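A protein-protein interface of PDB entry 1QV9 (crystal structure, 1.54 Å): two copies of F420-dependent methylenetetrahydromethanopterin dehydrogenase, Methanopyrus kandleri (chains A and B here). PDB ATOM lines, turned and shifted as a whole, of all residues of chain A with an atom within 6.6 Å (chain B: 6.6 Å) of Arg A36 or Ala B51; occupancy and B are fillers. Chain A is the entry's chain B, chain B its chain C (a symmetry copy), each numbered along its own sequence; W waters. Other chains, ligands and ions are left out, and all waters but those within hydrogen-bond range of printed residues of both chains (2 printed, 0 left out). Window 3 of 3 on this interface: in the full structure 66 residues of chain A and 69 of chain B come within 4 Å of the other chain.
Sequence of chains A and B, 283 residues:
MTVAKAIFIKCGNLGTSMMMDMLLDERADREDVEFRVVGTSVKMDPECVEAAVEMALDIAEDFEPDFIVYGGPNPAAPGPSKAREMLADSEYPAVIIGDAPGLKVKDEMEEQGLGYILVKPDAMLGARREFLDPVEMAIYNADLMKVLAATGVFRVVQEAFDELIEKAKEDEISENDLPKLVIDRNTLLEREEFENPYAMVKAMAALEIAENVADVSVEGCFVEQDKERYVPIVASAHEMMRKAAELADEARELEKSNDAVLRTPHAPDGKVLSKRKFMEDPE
Water W1 bridges the backbone carbonyl oxygen of Thr B40 (2.6 Å) and the backbone NH of Phe A35 (3.0 Å). Water W2 lies within hydrogen-bond range of the backbone carbonyl oxygen (O) of Asp A21 and the side-chain hydroxyl (OG) of Ser B41.
Of the printed residues of chain B, Arg A36 touches Gly B39 (3.6 Å), Ala B51 (3.6 Å) and Met B55 (3.6 Å). Of chain A, only Arg A36 (3.6 Å) comes within 4 Å of Ala B51. Of the printed residues of chain A, Ser B41 touches Asp A21. Of the printed residues of chain B, Val A37 touches Gly B39 (2.9 Å). Cys B48 touches none of the printed residues of chain A. Ile A7 touches none of the printed residues of chain B. The nearest residue of chain A that does not touch Ala B51 is Glu A34 (5.9 Å). The nearest printed residue of chain A that does not touch Met B55 is Ile A59 (4.3 Å).
The side-chain carboxylate of Asp A21 is in hydrogen-bond range of the side-chain hydroxyl of Ser B41. The backbone NH (N) of Val A37 sits at hydrogen-bond distance from the backbone carbonyl oxygen (O) of Gly B39 (2.9 Å).
The backbone carbonyl oxygen (O) of Arg A36 lies within hydrogen-bond range of the backbone NH (N) of Phe A8, at 2.8 Å. The guanidinium group (NH2) of Arg A36 lies within salt-bridge range of the side-chain carboxylate (OE1) of Glu A34 (2.7 Å). N of Arg A36 sits at hydrogen-bond distance from O of Ala A6.
No position is printed for both chains.
Hydrophobic or aromatic side chains of chain A within 4 Å of the printed part of chain B: Val A37. Hydrophobic or aromatic side chains of chain B within 4 Å of the printed part of chain A: Ala B51 and Met B55. Among the printed residues, 6 pairs touch across the chains. Among the printed residues, no Asp or Glu carboxylate lies within 4 Å of a Lys or Arg side-chain nitrogen of the other chain.
Phe A35 touches Thr B40 (O to CA, 3.6 Å). Arg A36 touches Gly B39 (CA to O, 3.6 Å). Arg A36 touches Ala B51. CD of Arg A36 touches SD of Met B55, 3.6 Å away.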
ATOM      1  N   ALA A   6     -32.688  11.825   0.225  1.00  0.00           N
ATOM      2  CA  ALA A   6     -31.576  11.208  -0.476  1.00  0.00           C
ATOM      3  C   ALA A   6     -30.481  12.221  -0.756  1.00  0.00           C
ATOM      4  O   ALA A   6     -30.733  13.424  -0.832  1.00  0.00           O
ATOM      5  CB  ALA A   6     -32.049  10.577  -1.796  1.00  0.00           C
ATOM      6  N   ILE A   7     -29.265  11.722  -0.880  1.00  0.00           N
ATOM      7  CA  ILE A   7     -28.127  12.560  -1.190  1.00  0.00           C
ATOM      8  C   ILE A   7     -27.589  12.081  -2.535  1.00  0.00           C
ATOM      9  O   ILE A   7     -27.416  10.886  -2.741  1.00  0.00           O
ATOM     10  CB  ILE A   7     -27.013  12.420  -0.155  1.00  0.00           C
ATOM     11  CG1 ILE A   7     -27.519  12.921   1.199  1.00  0.00           C
ATOM     12  CG2 ILE A   7     -25.778  13.165  -0.631  1.00  0.00           C
ATOM     13  CD1 ILE A   7     -26.483  12.890   2.290  1.00  0.00           C
ATOM     14  N   PHE A   8     -27.342  13.014  -3.452  1.00  0.00           N
ATOM     15  CA  PHE A   8     -26.795  12.645  -4.755  1.00  0.00           C
ATOM     16  C   PHE A   8     -25.368  13.149  -4.814  1.00  0.00           C
ATOM     17  O   PHE A   8     -25.109  14.299  -4.470  1.00  0.00           O
ATOM     18  CB  PHE A   8     -27.597  13.285  -5.900  1.00  0.00           C
ATOM     19  CG  PHE A   8     -28.987  12.740  -6.051  1.00  0.00           C
ATOM     20  CD1 PHE A   8     -30.037  13.219  -5.264  1.00  0.00           C
ATOM     21  CD2 PHE A   8     -29.257  11.747  -6.988  1.00  0.00           C
ATOM     22  CE1 PHE A   8     -31.320  12.721  -5.409  1.00  0.00           C
ATOM     23  CE2 PHE A   8     -30.540  11.237  -7.141  1.00  0.00           C
ATOM     24  CZ  PHE A   8     -31.582  11.728  -6.344  1.00  0.00           C
ATOM     25  N   ILE A   9     -24.444  12.293  -5.241  1.00  0.00           N
ATOM     26  CA  ILE A   9     -23.049  12.660  -5.361  1.00  0.00           C
ATOM     27  C   ILE A   9     -22.680  12.626  -6.846  1.00  0.00           C
ATOM     28  O   ILE A   9     -22.859  11.604  -7.508  1.00  0.00           O
ATOM     29  CB  ILE A   9     -22.121  11.664  -4.657  1.00  0.00           C
ATOM     30  CG1 ILE A   9     -22.566  11.476  -3.203  1.00  0.00           C
ATOM     31  CG2 ILE A   9     -20.685  12.161  -4.737  1.00  0.00           C
ATOM     32  CD1 ILE A   9     -21.868  10.316  -2.507  1.00  0.00           C
ATOM     33  N   ASP A  21     -31.399  13.862 -10.335  1.00  0.00           N
ATOM     34  CA  ASP A  21     -32.188  14.393  -9.222  1.00  0.00           C
ATOM     35  C   ASP A  21     -33.362  15.262  -9.646  1.00  0.00           C
ATOM     36  O   ASP A  21     -34.442  15.212  -9.038  1.00  0.00           O
ATOM     37  CB  ASP A  21     -31.276  15.164  -8.253  1.00  0.00           C
ATOM     38  CG  ASP A  21     -30.487  16.274  -8.935  1.00  0.00           C
ATOM     39  OD1 ASP A  21     -29.635  15.955  -9.798  1.00  0.00           O
ATOM     40  OD2 ASP A  21     -30.716  17.463  -8.613  1.00  0.00           O
ATOM     41  N   GLU A  34     -36.931  15.283  -0.184  1.00  0.00           N
ATOM     42  CA  GLU A  34     -35.992  16.346   0.126  1.00  0.00           C
ATOM     43  C   GLU A  34     -34.649  15.804  -0.318  1.00  0.00           C
ATOM     44  O   GLU A  34     -34.305  14.675   0.019  1.00  0.00           O
ATOM     45  CB  GLU A  34     -35.932  16.649   1.621  1.00  0.00           C
ATOM     46  CG  GLU A  34     -34.833  17.662   1.918  1.00  0.00           C
ATOM     47  CD  GLU A  34     -34.758  18.070   3.372  1.00  0.00           C
ATOM     48  OE1 GLU A  34     -33.939  18.963   3.687  1.00  0.00           O
ATOM     49  OE2 GLU A  34     -35.508  17.503   4.193  1.00  0.00           O
ATOM     50  N   PHE A  35     -33.882  16.600  -1.061  1.00  0.00           N
ATOM     51  CA  PHE A  35     -32.598  16.138  -1.566  1.00  0.00           C
ATOM     52  C   PHE A  35     -31.434  17.059  -1.279  1.00  0.00           C
ATOM     53  O   PHE A  35     -31.599  18.259  -1.078  1.00  0.00           O
ATOM     54  CB  PHE A  35     -32.643  15.982  -3.106  1.00  0.00           C
ATOM     55  CG  PHE A  35     -33.738  15.083  -3.615  1.00  0.00           C
ATOM     56  CD1 PHE A  35     -34.516  15.467  -4.714  1.00  0.00           C
ATOM     57  CD2 PHE A  35     -33.967  13.835  -3.037  1.00  0.00           C
ATOM     58  CE1 PHE A  35     -35.505  14.623  -5.227  1.00  0.00           C
ATOM     59  CE2 PHE A  35     -34.949  12.987  -3.540  1.00  0.00           C
ATOM     60  CZ  PHE A  35     -35.723  13.381  -4.644  1.00  0.00           C
ATOM     61  N   ARG A  36     -30.242  16.483  -1.291  1.00  0.00           N
ATOM     62  CA  ARG A  36     -29.009  17.249  -1.147  1.00  0.00           C
ATOM     63  C   ARG A  36     -28.109  16.741  -2.268  1.00  0.00           C
ATOM     64  O   ARG A  36     -28.081  15.549  -2.544  1.00  0.00           O
ATOM     65  CB  ARG A  36     -28.352  16.998   0.209  1.00  0.00           C
ATOM     66  CG  ARG A  36     -29.130  17.588   1.366  1.00  0.00           C
ATOM     67  CD  ARG A  36     -29.159  19.104   1.289  1.00  0.00           C
ATOM     68  NE  ARG A  36     -29.685  19.671   2.523  1.00  0.00           N
ATOM     69  CZ  ARG A  36     -30.971  19.666   2.858  1.00  0.00           C
ATOM     70  NH1 ARG A  36     -31.356  20.194   4.014  1.00  0.00           N
ATOM     71  NH2 ARG A  36     -31.871  19.160   2.029  1.00  0.00           N
ATOM     72  N   VAL A  37     -27.391  17.644  -2.923  1.00  0.00           N
ATOM     73  CA  VAL A  37     -26.506  17.262  -4.012  1.00  0.00           C
ATOM     74  C   VAL A  37     -25.113  17.790  -3.714  1.00  0.00           C
ATOM     75  O   VAL A  37     -24.951  18.948  -3.367  1.00  0.00           O
ATOM     76  CB  VAL A  37     -27.010  17.850  -5.372  1.00  0.00           C
ATOM     77  CG1 VAL A  37     -26.147  17.338  -6.522  1.00  0.00           C
ATOM     78  CG2 VAL A  37     -28.454  17.467  -5.593  1.00  0.00           C
ATOM     79  N   VAL A  38     -24.108  16.931  -3.839  1.00  0.00           N
ATOM     80  CA  VAL A  38     -22.730  17.331  -3.597  1.00  0.00           C
ATOM     81  C   VAL A  38     -21.777  16.668  -4.600  1.00  0.00           C
ATOM     82  O   VAL A  38     -22.084  15.609  -5.148  1.00  0.00           O
ATOM     83  CB  VAL A  38     -22.271  16.951  -2.158  1.00  0.00           C
ATOM     84  CG1 VAL A  38     -23.244  17.543  -1.132  1.00  0.00           C
ATOM     85  CG2 VAL A  38     -22.211  15.434  -2.009  1.00  0.00           C
ATOM     86  N   ILE A  59     -22.721  15.056   5.783  1.00  0.00           N
ATOM     87  CA  ILE A  59     -24.046  15.659   5.901  1.00  0.00           C
ATOM     88  C   ILE A  59     -25.140  14.626   6.205  1.00  0.00           C
ATOM     89  O   ILE A  59     -26.205  14.970   6.723  1.00  0.00           O
ATOM     90  CB  ILE A  59     -24.421  16.450   4.604  1.00  0.00           C
ATOM     91  CG1 ILE A  59     -24.685  15.484   3.458  1.00  0.00           C
ATOM     92  CG2 ILE A  59     -23.279  17.391   4.204  1.00  0.00           C
ATOM     93  CD1 ILE A  59     -25.145  16.165   2.185  1.00  0.00           C
ATOM     94  N   PHE A  63     -28.673  14.915   8.122  1.00  0.00           N
ATOM     95  CA  PHE A  63     -29.710  14.864   7.106  1.00  0.00           C
ATOM     96  C   PHE A  63     -30.472  13.552   7.162  1.00  0.00           C
ATOM     97  O   PHE A  63     -31.686  13.517   6.959  1.00  0.00           O
ATOM     98  CB  PHE A  63     -29.089  15.062   5.724  1.00  0.00           C
ATOM     99  CG  PHE A  63     -30.093  15.237   4.629  1.00  0.00           C
ATOM    100  CD1 PHE A  63     -30.992  16.296   4.654  1.00  0.00           C
ATOM    101  CD2 PHE A  63     -30.120  14.357   3.551  1.00  0.00           C
ATOM    102  CE1 PHE A  63     -31.904  16.480   3.620  1.00  0.00           C
ATOM    103  CE2 PHE A  63     -31.029  14.532   2.510  1.00  0.00           C
ATOM    104  CZ  PHE A  63     -31.920  15.591   2.541  1.00  0.00           C
ATOM    105  N   GLY B  39     -25.871  21.806  -3.258  1.00  0.00           N
ATOM    106  CA  GLY B  39     -27.164  22.388  -3.530  1.00  0.00           C
ATOM    107  C   GLY B  39     -28.306  21.516  -3.055  1.00  0.00           C
ATOM    108  O   GLY B  39     -28.098  20.422  -2.526  1.00  0.00           O
ATOM    109  N   THR B  40     -29.518  22.013  -3.252  1.00  0.00           N
ATOM    110  CA  THR B  40     -30.715  21.315  -2.830  1.00  0.00           C
ATOM    111  C   THR B  40     -31.567  20.890  -4.010  1.00  0.00           C
ATOM    112  O   THR B  40     -32.787  20.766  -3.897  1.00  0.00           O
ATOM    113  CB  THR B  40     -31.538  22.223  -1.916  1.00  0.00           C
ATOM    114  OG1 THR B  40     -31.735  23.485  -2.568  1.00  0.00           O
ATOM    115  CG2 THR B  40     -30.794  22.453  -0.601  1.00  0.00           C
ATOM    116  N   SER B  41     -30.907  20.672  -5.147  1.00  0.00           N
ATOM    117  CA  SER B  41     -31.585  20.273  -6.363  1.00  0.00           C
ATOM    118  C   SER B  41     -32.479  21.427  -6.830  1.00  0.00           C
ATOM    119  O   SER B  41     -32.082  22.593  -6.742  1.00  0.00           O
ATOM    120  CB  SER B  41     -32.392  18.989  -6.123  1.00  0.00           C
ATOM    121  OG  SER B  41     -32.818  18.412  -7.348  1.00  0.00           O
ATOM    122  N   PRO B  46     -36.766  29.616   0.777  1.00  0.00           N
ATOM    123  CA  PRO B  46     -35.872  30.121   1.825  1.00  0.00           C
ATOM    124  C   PRO B  46     -35.229  29.046   2.712  1.00  0.00           C
ATOM    125  O   PRO B  46     -34.038  29.119   3.011  1.00  0.00           O
ATOM    126  CB  PRO B  46     -36.774  31.077   2.607  1.00  0.00           C
ATOM    127  CG  PRO B  46     -37.664  31.632   1.533  1.00  0.00           C
ATOM    128  CD  PRO B  46     -38.025  30.385   0.742  1.00  0.00           C
ATOM    129  N   GLU B  47     -36.006  28.050   3.130  1.00  0.00           N
ATOM    130  CA  GLU B  47     -35.472  26.977   3.974  1.00  0.00           C
ATOM    131  C   GLU B  47     -34.349  26.208   3.273  1.00  0.00           C
ATOM    132  O   GLU B  47     -33.253  26.023   3.821  1.00  0.00           O
ATOM    133  CB  GLU B  47     -36.573  25.979   4.334  1.00  0.00           C
ATOM    134  CG  GLU B  47     -37.699  26.533   5.178  1.00  0.00           C
ATOM    135  CD  GLU B  47     -38.878  25.576   5.256  1.00  0.00           C
ATOM    136  OE1 GLU B  47     -39.586  25.418   4.234  1.00  0.00           O
ATOM    137  OE2 GLU B  47     -39.091  24.976   6.334  1.00  0.00           O
ATOM    138  N   CYS B  48     -34.637  25.752   2.058  1.00  0.00           N
ATOM    139  CA  CYS B  48     -33.668  24.983   1.293  1.00  0.00           C
ATOM    140  C   CYS B  48     -32.430  25.768   0.922  1.00  0.00           C
ATOM    141  O   CYS B  48     -31.327  25.254   1.036  1.00  0.00           O
ATOM    142  CB  CYS B  48     -34.333  24.405   0.047  1.00  0.00           C
ATOM    143  SG  CYS B  48     -35.414  22.991   0.410  1.00  0.00           S
ATOM    144  N   VAL B  49     -32.605  27.008   0.471  1.00  0.00           N
ATOM    145  CA  VAL B  49     -31.456  27.823   0.115  1.00  0.00           C
ATOM    146  C   VAL B  49     -30.593  28.089   1.342  1.00  0.00           C
ATOM    147  O   VAL B  49     -29.373  28.156   1.243  1.00  0.00           O
ATOM    148  CB  VAL B  49     -31.880  29.168  -0.503  1.00  0.00           C
ATOM    149  CG1 VAL B  49     -30.663  30.024  -0.779  1.00  0.00           C
ATOM    150  CG2 VAL B  49     -32.655  28.919  -1.795  1.00  0.00           C
ATOM    151  N   GLU B  50     -31.210  28.241   2.512  1.00  0.00           N
ATOM    152  CA  GLU B  50     -30.404  28.491   3.706  1.00  0.00           C
ATOM    153  C   GLU B  50     -29.556  27.263   3.968  1.00  0.00           C
ATOM    154  O   GLU B  50     -28.348  27.363   4.186  1.00  0.00           O
ATOM    155  CB  GLU B  50     -31.292  28.798   4.923  1.00  0.00           C
ATOM    156  CG  GLU B  50     -30.506  29.238   6.148  1.00  0.00           C
ATOM    157  CD  GLU B  50     -31.394  29.755   7.267  1.00  0.00           C
ATOM    158  OE1 GLU B  50     -30.877  30.490   8.138  1.00  0.00           O
ATOM    159  OE2 GLU B  50     -32.600  29.424   7.280  1.00  0.00           O
ATOM    160  N   ALA B  51     -30.190  26.102   3.939  1.00  0.00           N
ATOM    161  CA  ALA B  51     -29.470  24.860   4.153  1.00  0.00           C
ATOM    162  C   ALA B  51     -28.339  24.752   3.125  1.00  0.00           C
ATOM    163  O   ALA B  51     -27.221  24.354   3.458  1.00  0.00           O
ATOM    164  CB  ALA B  51     -30.416  23.670   4.019  1.00  0.00           C
ATOM    165  N   ALA B  52     -28.633  25.118   1.874  1.00  0.00           N
ATOM    166  CA  ALA B  52     -27.633  25.041   0.808  1.00  0.00           C
ATOM    167  C   ALA B  52     -26.407  25.890   1.112  1.00  0.00           C
ATOM    168  O   ALA B  52     -25.279  25.412   1.012  1.00  0.00           O
ATOM    169  CB  ALA B  52     -28.260  25.471  -0.543  1.00  0.00           C
ATOM    170  N   VAL B  53     -26.624  27.143   1.492  1.00  0.00           N
ATOM    171  CA  VAL B  53     -25.511  28.033   1.808  1.00  0.00           C
ATOM    172  C   VAL B  53     -24.775  27.595   3.083  1.00  0.00           C
ATOM    173  O   VAL B  53     -23.563  27.772   3.196  1.00  0.00           O
ATOM    174  CB  VAL B  53     -25.979  29.487   1.960  1.00  0.00           C
ATOM    175  CG1 VAL B  53     -24.774  30.391   2.122  1.00  0.00           C
ATOM    176  CG2 VAL B  53     -26.768  29.916   0.723  1.00  0.00           C
ATOM    177  N   GLU B  54     -25.503  27.010   4.029  1.00  0.00           N
ATOM    178  CA  GLU B  54     -24.871  26.529   5.263  1.00  0.00           C
ATOM    179  C   GLU B  54     -23.857  25.446   4.905  1.00  0.00           C
ATOM    180  O   GLU B  54     -22.701  25.499   5.345  1.00  0.00           O
ATOM    181  CB  GLU B  54     -25.903  25.936   6.214  1.00  0.00           C
ATOM    182  CG  GLU B  54     -26.954  26.905   6.717  1.00  0.00           C
ATOM    183  CD  GLU B  54     -27.795  26.282   7.816  1.00  0.00           C
ATOM    184  OE1 GLU B  54     -27.248  26.073   8.920  1.00  0.00           O
ATOM    185  OE2 GLU B  54     -28.991  25.988   7.572  1.00  0.00           O
ATOM    186  N   MET B  55     -24.297  24.463   4.109  1.00  0.00           N
ATOM    187  CA  MET B  55     -23.427  23.364   3.663  1.00  0.00           C
ATOM    188  C   MET B  55     -22.161  23.983   3.090  1.00  0.00           C
ATOM    189  O   MET B  55     -21.046  23.639   3.484  1.00  0.00           O
ATOM    190  CB  MET B  55     -24.079  22.516   2.546  1.00  0.00           C
ATOM    191  CG  MET B  55     -25.209  21.544   2.938  1.00  0.00           C
ATOM    192  SD  MET B  55     -25.787  20.355   1.440  1.00  0.00           S
ATOM    193  CE  MET B  55     -26.359  21.726   0.200  1.00  0.00           C
ATOM    194  N   ALA B  56     -22.351  24.899   2.144  1.00  0.00           N
ATOM    195  CA  ALA B  56     -21.244  25.571   1.493  1.00  0.00           C
ATOM    196  C   ALA B  56     -20.316  26.256   2.488  1.00  0.00           C
ATOM    197  O   ALA B  56     -19.102  26.059   2.440  1.00  0.00           O
ATOM    198  CB  ALA B  56     -21.776  26.600   0.480  1.00  0.00           C
ATOM    199  N   MET B  86     -26.672  36.080   3.051  1.00  0.00           N
ATOM    200  CA  MET B  86     -25.734  35.169   3.715  1.00  0.00           C
ATOM    201  C   MET B  86     -24.318  35.255   3.131  1.00  0.00           C
ATOM    202  O   MET B  86     -23.336  35.292   3.867  1.00  0.00           O
ATOM    203  CB  MET B  86     -26.259  33.720   3.646  1.00  0.00           C
ATOM    204  CG  MET B  86     -27.565  33.491   4.415  1.00  0.00           C
ATOM    205  SD  MET B  86     -28.437  31.749   4.279  1.00  0.00           S
ATOM    206  CE  MET B  86     -27.543  30.817   5.742  1.00  0.00           C
HETATM  207  O   HOH W   1     -34.335  18.978  -2.796  1.00  0.00           O
HETATM  208  O   HOH W   2     -35.339  17.203  -7.429  1.00  0.00           O
